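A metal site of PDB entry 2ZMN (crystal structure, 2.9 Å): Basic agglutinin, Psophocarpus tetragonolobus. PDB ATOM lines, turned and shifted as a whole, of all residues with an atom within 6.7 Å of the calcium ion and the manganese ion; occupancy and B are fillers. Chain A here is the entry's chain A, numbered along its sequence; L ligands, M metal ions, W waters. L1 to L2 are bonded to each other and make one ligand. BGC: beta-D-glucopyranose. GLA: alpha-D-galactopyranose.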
ATOM      1  N   ASP A  87     -14.860  19.496  14.632  1.00  0.00           N
ATOM      2  CA  ASP A  87     -14.187  20.781  14.653  1.00  0.00           C
ATOM      3  C   ASP A  87     -12.648  20.650  14.745  1.00  0.00           C
ATOM      4  O   ASP A  87     -11.898  21.598  14.456  1.00  0.00           O
ATOM      5  CB  ASP A  87     -14.685  21.611  15.832  1.00  0.00           C
ATOM      6  CG  ASP A  87     -16.002  22.297  15.567  1.00  0.00           C
ATOM      7  OD1 ASP A  87     -17.063  21.673  15.757  1.00  0.00           O
ATOM      8  OD2 ASP A  87     -15.974  23.465  15.152  1.00  0.00           O
ATOM      9  N   GLY A 104     -17.727  22.259  20.156  1.00  0.00           N
ATOM     10  CA  GLY A 104     -17.573  22.993  18.915  1.00  0.00           C
ATOM     11  C   GLY A 104     -16.194  23.576  18.710  1.00  0.00           C
ATOM     12  O   GLY A 104     -15.191  22.893  18.937  1.00  0.00           O
ATOM     13  N   GLY A 105     -16.135  24.829  18.297  1.00  0.00           N
ATOM     14  CA  GLY A 105     -14.871  25.492  18.057  1.00  0.00           C
ATOM     15  C   GLY A 105     -14.011  25.688  19.296  1.00  0.00           C
ATOM     16  O   GLY A 105     -12.921  26.231  19.237  1.00  0.00           O
ATOM     17  N   TYR A 106     -14.499  25.245  20.450  1.00  0.00           N
ATOM     18  CA  TYR A 106     -13.736  25.388  21.672  1.00  0.00           C
ATOM     19  C   TYR A 106     -13.026  24.094  22.037  1.00  0.00           C
ATOM     20  O   TYR A 106     -12.330  24.027  23.069  1.00  0.00           O
ATOM     21  CB  TYR A 106     -14.622  25.860  22.802  1.00  0.00           C
ATOM     22  CG  TYR A 106     -15.096  27.270  22.589  1.00  0.00           C
ATOM     23  CD1 TYR A 106     -14.185  28.307  22.475  1.00  0.00           C
ATOM     24  CD2 TYR A 106     -16.442  27.576  22.487  1.00  0.00           C
ATOM     25  CE1 TYR A 106     -14.597  29.613  22.265  1.00  0.00           C
ATOM     26  CE2 TYR A 106     -16.876  28.887  22.278  1.00  0.00           C
ATOM     27  CZ  TYR A 106     -15.940  29.897  22.167  1.00  0.00           C
ATOM     28  OH  TYR A 106     -16.352  31.203  21.957  1.00  0.00           O
ATOM     29  N   PHE A 107     -13.207  23.072  21.202  1.00  0.00           N
ATOM     30  CA  PHE A 107     -12.557  21.775  21.385  1.00  0.00           C
ATOM     31  C   PHE A 107     -12.781  21.087  22.734  1.00  0.00           C
ATOM     32  O   PHE A 107     -12.245  20.009  22.964  1.00  0.00           O
ATOM     33  CB  PHE A 107     -11.055  21.925  21.167  1.00  0.00           C
ATOM     34  CG  PHE A 107     -10.685  22.687  19.932  1.00  0.00           C
ATOM     35  CD1 PHE A 107     -10.970  22.197  18.680  1.00  0.00           C
ATOM     36  CD2 PHE A 107     -10.008  23.887  20.039  1.00  0.00           C
ATOM     37  CE1 PHE A 107     -10.581  22.897  17.539  1.00  0.00           C
ATOM     38  CE2 PHE A 107      -9.630  24.583  18.906  1.00  0.00           C
ATOM     39  CZ  PHE A 107      -9.914  24.077  17.646  1.00  0.00           C
ATOM     40  N   GLU A 122      -3.366  23.008  18.480  1.00  0.00           N
ATOM     41  CA  GLU A 122      -4.593  22.570  17.852  1.00  0.00           C
ATOM     42  C   GLU A 122      -4.461  22.171  16.414  1.00  0.00           C
ATOM     43  O   GLU A 122      -3.619  22.674  15.687  1.00  0.00           O
ATOM     44  CB  GLU A 122      -5.655  23.675  17.934  1.00  0.00           C
ATOM     45  CG  GLU A 122      -5.259  24.891  17.141  1.00  0.00           C
ATOM     46  CD  GLU A 122      -6.339  25.943  17.052  1.00  0.00           C
ATOM     47  OE1 GLU A 122      -6.807  26.453  18.098  1.00  0.00           O
ATOM     48  OE2 GLU A 122      -6.726  26.269  15.916  1.00  0.00           O
ATOM     49  N   ASP A 124      -7.025  22.288  13.802  1.00  0.00           N
ATOM     50  CA  ASP A 124      -8.326  22.841  13.481  1.00  0.00           C
ATOM     51  C   ASP A 124      -8.853  22.520  12.103  1.00  0.00           C
ATOM     52  O   ASP A 124      -8.189  22.801  11.105  1.00  0.00           O
ATOM     53  CB  ASP A 124      -8.257  24.352  13.642  1.00  0.00           C
ATOM     54  CG  ASP A 124      -9.595  24.970  14.011  1.00  0.00           C
ATOM     55  OD1 ASP A 124     -10.642  24.403  13.612  1.00  0.00           O
ATOM     56  OD2 ASP A 124      -9.577  26.019  14.699  1.00  0.00           O
ATOM     57  N   THR A 125     -10.064  21.985  12.043  1.00  0.00           N
ATOM     58  CA  THR A 125     -10.681  21.606  10.782  1.00  0.00           C
ATOM     59  C   THR A 125     -11.886  22.453  10.367  1.00  0.00           C
ATOM     60  O   THR A 125     -12.347  22.364   9.223  1.00  0.00           O
ATOM     61  CB  THR A 125     -11.098  20.143  10.830  1.00  0.00           C
ATOM     62  OG1 THR A 125     -11.953  19.928  11.963  1.00  0.00           O
ATOM     63  CG2 THR A 125      -9.876  19.258  10.984  1.00  0.00           C
ATOM     64  N   PHE A 126     -12.405  23.275  11.277  1.00  0.00           N
ATOM     65  CA  PHE A 126     -13.547  24.144  10.987  1.00  0.00           C
ATOM     66  C   PHE A 126     -13.156  25.593  11.136  1.00  0.00           C
ATOM     67  O   PHE A 126     -12.463  25.954  12.088  1.00  0.00           O
ATOM     68  CB  PHE A 126     -14.707  23.875  11.920  1.00  0.00           C
ATOM     69  CG  PHE A 126     -15.892  24.715  11.643  1.00  0.00           C
ATOM     70  CD1 PHE A 126     -16.736  24.425  10.571  1.00  0.00           C
ATOM     71  CD2 PHE A 126     -16.176  25.818  12.432  1.00  0.00           C
ATOM     72  CE1 PHE A 126     -17.844  25.223  10.292  1.00  0.00           C
ATOM     73  CE2 PHE A 126     -17.285  26.616  12.153  1.00  0.00           C
ATOM     74  CZ  PHE A 126     -18.114  26.309  11.077  1.00  0.00           C
ATOM     75  N   ARG A 127     -13.617  26.453  10.224  1.00  0.00           N
ATOM     76  CA  ARG A 127     -13.278  27.871  10.305  1.00  0.00           C
ATOM     77  C   ARG A 127     -14.288  28.739  11.061  1.00  0.00           C
ATOM     78  O   ARG A 127     -15.347  29.071  10.542  1.00  0.00           O
ATOM     79  CB  ARG A 127     -13.063  28.438   8.912  1.00  0.00           C
ATOM     80  CG  ARG A 127     -12.597  29.868   8.966  1.00  0.00           C
ATOM     81  CD  ARG A 127     -12.137  30.376   7.624  1.00  0.00           C
ATOM     82  NE  ARG A 127     -11.543  31.702   7.761  1.00  0.00           N
ATOM     83  CZ  ARG A 127     -11.017  32.402   6.763  1.00  0.00           C
ATOM     84  NH1 ARG A 127     -11.015  31.897   5.533  1.00  0.00           N
ATOM     85  NH2 ARG A 127     -10.489  33.587   7.001  1.00  0.00           N
ATOM     86  N   ASN A 128     -13.942  29.110  12.283  1.00  0.00           N
ATOM     87  CA  ASN A 128     -14.798  29.964  13.088  1.00  0.00           C
ATOM     88  C   ASN A 128     -14.509  31.408  12.697  1.00  0.00           C
ATOM     89  O   ASN A 128     -13.654  31.668  11.849  1.00  0.00           O
ATOM     90  CB  ASN A 128     -14.539  29.755  14.573  1.00  0.00           C
ATOM     91  CG  ASN A 128     -15.090  28.431  15.081  1.00  0.00           C
ATOM     92  OD1 ASN A 128     -14.651  27.374  14.659  1.00  0.00           O
ATOM     93  ND2 ASN A 128     -16.060  28.491  15.970  1.00  0.00           N
ATOM     94  N   TRP A 130     -12.947  33.625  14.209  1.00  0.00           N
ATOM     95  CA  TRP A 130     -11.580  33.981  14.593  1.00  0.00           C
ATOM     96  C   TRP A 130     -10.477  33.179  13.929  1.00  0.00           C
ATOM     97  O   TRP A 130      -9.308  33.366  14.237  1.00  0.00           O
ATOM     98  CB  TRP A 130     -11.439  33.835  16.101  1.00  0.00           C
ATOM     99  CG  TRP A 130     -11.715  32.451  16.553  1.00  0.00           C
ATOM    100  CD1 TRP A 130     -10.880  31.365  16.445  1.00  0.00           C
ATOM    101  CD2 TRP A 130     -12.925  31.951  17.142  1.00  0.00           C
ATOM    102  NE1 TRP A 130     -11.485  30.226  16.932  1.00  0.00           N
ATOM    103  CE2 TRP A 130     -12.747  30.560  17.362  1.00  0.00           C
ATOM    104  CE3 TRP A 130     -14.141  32.539  17.512  1.00  0.00           C
ATOM    105  CZ2 TRP A 130     -13.742  29.761  17.935  1.00  0.00           C
ATOM    106  CZ3 TRP A 130     -15.129  31.737  18.081  1.00  0.00           C
ATOM    107  CH2 TRP A 130     -14.922  30.367  18.287  1.00  0.00           C
ATOM    108  N   ASP A 131     -10.840  32.284  13.004  1.00  0.00           N
ATOM    109  CA  ASP A 131      -9.883  31.413  12.335  1.00  0.00           C
ATOM    110  C   ASP A 131      -9.426  31.788  10.974  1.00  0.00           C
ATOM    111  O   ASP A 131     -10.155  32.383  10.225  1.00  0.00           O
ATOM    112  CB  ASP A 131     -10.435  29.983  12.190  1.00  0.00           C
ATOM    113  CG  ASP A 131     -10.380  29.199  13.480  1.00  0.00           C
ATOM    114  OD1 ASP A 131      -9.415  29.360  14.271  1.00  0.00           O
ATOM    115  OD2 ASP A 131     -11.289  28.396  13.683  1.00  0.00           O
ATOM    116  N   PRO A 132      -8.193  31.426  10.635  1.00  0.00           N
ATOM    117  CA  PRO A 132      -7.628  31.694   9.320  1.00  0.00           C
ATOM    118  C   PRO A 132      -8.138  30.505   8.511  1.00  0.00           C
ATOM    119  O   PRO A 132      -8.886  29.705   9.041  1.00  0.00           O
ATOM    120  CB  PRO A 132      -6.129  31.645   9.565  1.00  0.00           C
ATOM    121  CG  PRO A 132      -5.997  30.695  10.666  1.00  0.00           C
ATOM    122  CD  PRO A 132      -7.113  31.101  11.586  1.00  0.00           C
ATOM    123  N   ILE A 134      -8.724  26.887   6.942  1.00  0.00           N
ATOM    124  CA  ILE A 134      -8.488  25.574   7.548  1.00  0.00           C
ATOM    125  C   ILE A 134      -8.255  24.497   6.498  1.00  0.00           C
ATOM    126  O   ILE A 134      -8.547  24.688   5.341  1.00  0.00           O
ATOM    127  CB  ILE A 134      -9.685  25.164   8.474  1.00  0.00           C
ATOM    128  CG1 ILE A 134     -11.023  25.220   7.732  1.00  0.00           C
ATOM    129  CG2 ILE A 134      -9.742  26.073   9.667  1.00  0.00           C
ATOM    130  CD1 ILE A 134     -11.226  24.127   6.759  1.00  0.00           C
ATOM    131  N   HIS A 136      -5.685  23.903   9.876  1.00  0.00           N
ATOM    132  CA  HIS A 136      -4.450  24.558  10.270  1.00  0.00           C
ATOM    133  C   HIS A 136      -3.996  24.128  11.653  1.00  0.00           C
ATOM    134  O   HIS A 136      -4.805  23.711  12.481  1.00  0.00           O
ATOM    135  CB  HIS A 136      -4.611  26.088  10.232  1.00  0.00           C
ATOM    136  CG  HIS A 136      -5.669  26.614  11.150  1.00  0.00           C
ATOM    137  ND1 HIS A 136      -6.823  27.213  10.690  1.00  0.00           N
ATOM    138  CD2 HIS A 136      -5.751  26.639  12.496  1.00  0.00           C
ATOM    139  CE1 HIS A 136      -7.561  27.591  11.723  1.00  0.00           C
ATOM    140  NE2 HIS A 136      -6.932  27.259  12.832  1.00  0.00           N
ATOM    141  N   ILE A 137      -2.689  24.217  11.873  1.00  0.00           N
ATOM    142  CA  ILE A 137      -2.093  23.900  13.163  1.00  0.00           C
ATOM    143  C   ILE A 137      -2.025  25.252  13.823  1.00  0.00           C
ATOM    144  O   ILE A 137      -1.726  26.259  13.161  1.00  0.00           O
ATOM    145  CB  ILE A 137      -0.645  23.417  13.064  1.00  0.00           C
ATOM    146  CG1 ILE A 137      -0.525  22.286  12.059  1.00  0.00           C
ATOM    147  CG2 ILE A 137      -0.178  22.916  14.423  1.00  0.00           C
ATOM    148  CD1 ILE A 137       0.895  21.869  11.797  1.00  0.00           C
ATOM    149  N   GLY A 138      -2.297  25.298  15.116  1.00  0.00           N
ATOM    150  CA  GLY A 138      -2.236  26.569  15.793  1.00  0.00           C
ATOM    151  C   GLY A 138      -1.721  26.393  17.195  1.00  0.00           C
ATOM    152  O   GLY A 138      -1.902  25.348  17.789  1.00  0.00           O
ATOM    153  N   ASP A 140      -2.095  27.741  20.888  1.00  0.00           N
ATOM    154  CA  ASP A 140      -3.004  28.492  21.736  1.00  0.00           C
ATOM    155  C   ASP A 140      -2.541  28.651  23.169  1.00  0.00           C
ATOM    156  O   ASP A 140      -2.060  27.716  23.791  1.00  0.00           O
ATOM    157  CB  ASP A 140      -4.389  27.829  21.746  1.00  0.00           C
ATOM    158  CG  ASP A 140      -4.911  27.525  20.360  1.00  0.00           C
ATOM    159  OD1 ASP A 140      -4.506  28.201  19.390  1.00  0.00           O
ATOM    160  OD2 ASP A 140      -5.734  26.616  20.263  1.00  0.00           O
ATOM    161  N   VAL A 144      -8.516  30.281  22.333  1.00  0.00           N
ATOM    162  CA  VAL A 144      -8.630  29.425  21.165  1.00  0.00           C
ATOM    163  C   VAL A 144      -8.270  30.252  19.942  1.00  0.00           C
ATOM    164  O   VAL A 144      -8.386  29.801  18.813  1.00  0.00           O
ATOM    165  CB  VAL A 144     -10.054  28.814  21.098  1.00  0.00           C
ATOM    166  CG1 VAL A 144     -10.877  29.437  19.980  1.00  0.00           C
ATOM    167  CG2 VAL A 144      -9.955  27.310  20.969  1.00  0.00           C
ATOM    168  N   ILE A 145      -7.839  31.494  20.178  1.00  0.00           N
ATOM    169  CA  ILE A 145      -7.430  32.390  19.100  1.00  0.00           C
ATOM    170  C   ILE A 145      -5.928  32.290  19.071  1.00  0.00           C
ATOM    171  O   ILE A 145      -5.236  33.011  19.777  1.00  0.00           O
ATOM    172  CB  ILE A 145      -7.808  33.818  19.404  1.00  0.00           C
ATOM    173  CG1 ILE A 145      -9.328  33.942  19.450  1.00  0.00           C
ATOM    174  CG2 ILE A 145      -7.243  34.748  18.335  1.00  0.00           C
ATOM    175  CD1 ILE A 145      -9.812  35.328  19.801  1.00  0.00           C
ATOM    176  N   SER A 146      -5.431  31.372  18.231  1.00  0.00           N
ATOM    177  CA  SER A 146      -3.989  31.065  18.095  1.00  0.00           C
ATOM    178  C   SER A 146      -3.057  32.252  18.019  1.00  0.00           C
ATOM    179  O   SER A 146      -3.396  33.267  17.450  1.00  0.00           O
ATOM    180  CB  SER A 146      -3.762  30.196  16.861  1.00  0.00           C
ATOM    181  OG  SER A 146      -4.661  29.111  16.832  1.00  0.00           O
ATOM    182  N   THR A 149      -0.056  30.432  13.548  1.00  0.00           N
ATOM    183  CA  THR A 149      -0.880  29.511  12.782  1.00  0.00           C
ATOM    184  C   THR A 149      -0.207  29.066  11.501  1.00  0.00           C
ATOM    185  O   THR A 149       0.502  29.849  10.891  1.00  0.00           O
ATOM    186  CB  THR A 149      -2.220  30.187  12.436  1.00  0.00           C
ATOM    187  OG1 THR A 149      -3.260  29.608  13.233  1.00  0.00           O
ATOM    188  CG2 THR A 149      -2.559  30.062  10.946  1.00  0.00           C
HETATM  189  C2  BGC L   1     -21.768  31.452  11.151  1.00  0.00           C
HETATM  190  C3  BGC L   1     -21.029  31.474  12.488  1.00  0.00           C
HETATM  191  C4  BGC L   1     -21.462  30.318  13.388  1.00  0.00           C
HETATM  192  C5  BGC L   1     -21.383  29.012  12.589  1.00  0.00           C
HETATM  193  C6  BGC L   1     -21.816  27.795  13.383  1.00  0.00           C
HETATM  194  C1  BGC L   1     -21.762  30.064  10.502  1.00  0.00           C
HETATM  195  O1  BGC L   1     -22.616  30.058   9.425  1.00  0.00           O
HETATM  196  O2  BGC L   1     -21.142  32.370  10.256  1.00  0.00           O
HETATM  197  O3  BGC L   1     -21.297  32.701  13.166  1.00  0.00           O
HETATM  198  O4  BGC L   1     -20.618  30.281  14.535  1.00  0.00           O
HETATM  199  O5  BGC L   1     -22.221  29.076  11.429  1.00  0.00           O
HETATM  200  O6  BGC L   1     -20.749  27.496  14.309  1.00  0.00           O
HETATM  201  C1  GLA L   2     -21.001  26.470  15.195  1.00  0.00           C
HETATM  202  C2  GLA L   2     -19.744  26.252  16.055  1.00  0.00           C
HETATM  203  C3  GLA L   2     -18.603  25.795  15.159  1.00  0.00           C
HETATM  204  C4  GLA L   2     -19.017  24.525  14.397  1.00  0.00           C
HETATM  205  C5  GLA L   2     -20.291  24.798  13.619  1.00  0.00           C
HETATM  206  C6  GLA L   2     -20.831  23.571  12.929  1.00  0.00           C
HETATM  207  O2  GLA L   2     -19.380  27.459  16.709  1.00  0.00           O
HETATM  208  O3  GLA L   2     -17.454  25.558  15.949  1.00  0.00           O
HETATM  209  O4  GLA L   2     -19.243  23.473  15.311  1.00  0.00           O
HETATM  210  O5  GLA L   2     -21.328  25.264  14.516  1.00  0.00           O
HETATM  211  O6  GLA L   2     -21.764  23.917  11.909  1.00  0.00           O
HETATM  212 CA    CA M   1     -12.205  26.261  14.588  1.00  0.00          CA
HETATM  213 MN    MN M   2      -8.017  27.743  14.793  1.00  0.00          MN
HETATM  214  O   HOH W   1     -13.656  24.268  15.775  1.00  0.00           O
HETATM  215  O   HOH W   2     -12.023  26.891  17.201  1.00  0.00           O
HETATM  216  O   HOH W   3      -9.041  27.601  16.804  1.00  0.00           O
HETATM  217  O   HOH W   4      -6.900  29.564  15.432  1.00  0.00           O
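The backbone carbonyl oxygen (O) of Asp 131 sits at hydrogen-bond distance from the guanidinium group (NE) of Arg 127 (2.9 Å).
The side-chain carboxylate of Asp 131 sits close to the indole nitrogen of Trp 130 (3.5 Å).
OD2 of Asp 140 sits close to OE1 of Glu 122 (2.4 Å).
The backbone NH of Glu 122 sits at hydrogen-bond distance from the backbone carbonyl oxygen of Gly 138 (2.8 Å).
The calcium ion is bound by OD2 of Asp 131 (2.5 Å), O of Phe 126 (2.5 Å), OD1 of Asp 124 (2.6 Å), OD2 of Asp 124 (2.6 Å), OD1 of Asn 128 (2.7 Å), water W2 (2.7 Å) and water W1 (2.7 Å).
Water W3 lies within hydrogen-bond range of OE1 of Glu 122 (2.8 Å) and O of Val 144 (3.1 Å).
The side-chain amide nitrogen (ND2) of Asn 128 sits at hydrogen-bond distance from an oxygen (O3) of GLA L2.
An oxygen (O3) of GLA L2 sits at hydrogen-bond distance from the backbone NH of Gly 105, at 2.8 Å.
OD2 of Asp 87 sits at hydrogen-bond distance from O3 of GLA L2 (2.7 Å).
The manganese ion is bound by OD1 of Asp 131 (2.2 Å), water W4 (2.2 Å), OE2 of Glu 122 (2.3 Å), water W3 (2.3 Å), NE2 of His 136 (2.3 Å) and OD2 of Asp 124 (2.3 Å).
The manganese ion has six donor atoms within binding distance.
Within 4 Å of the manganese ion: Glu 122, Asp 124, Asp 131 and His 136.
The nearest printed residue that does not touch the manganese ion is Ser 146 (4.2 Å).
The nearest printed residue that does not touch the calcium ion is Phe 107 (4.4 Å).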
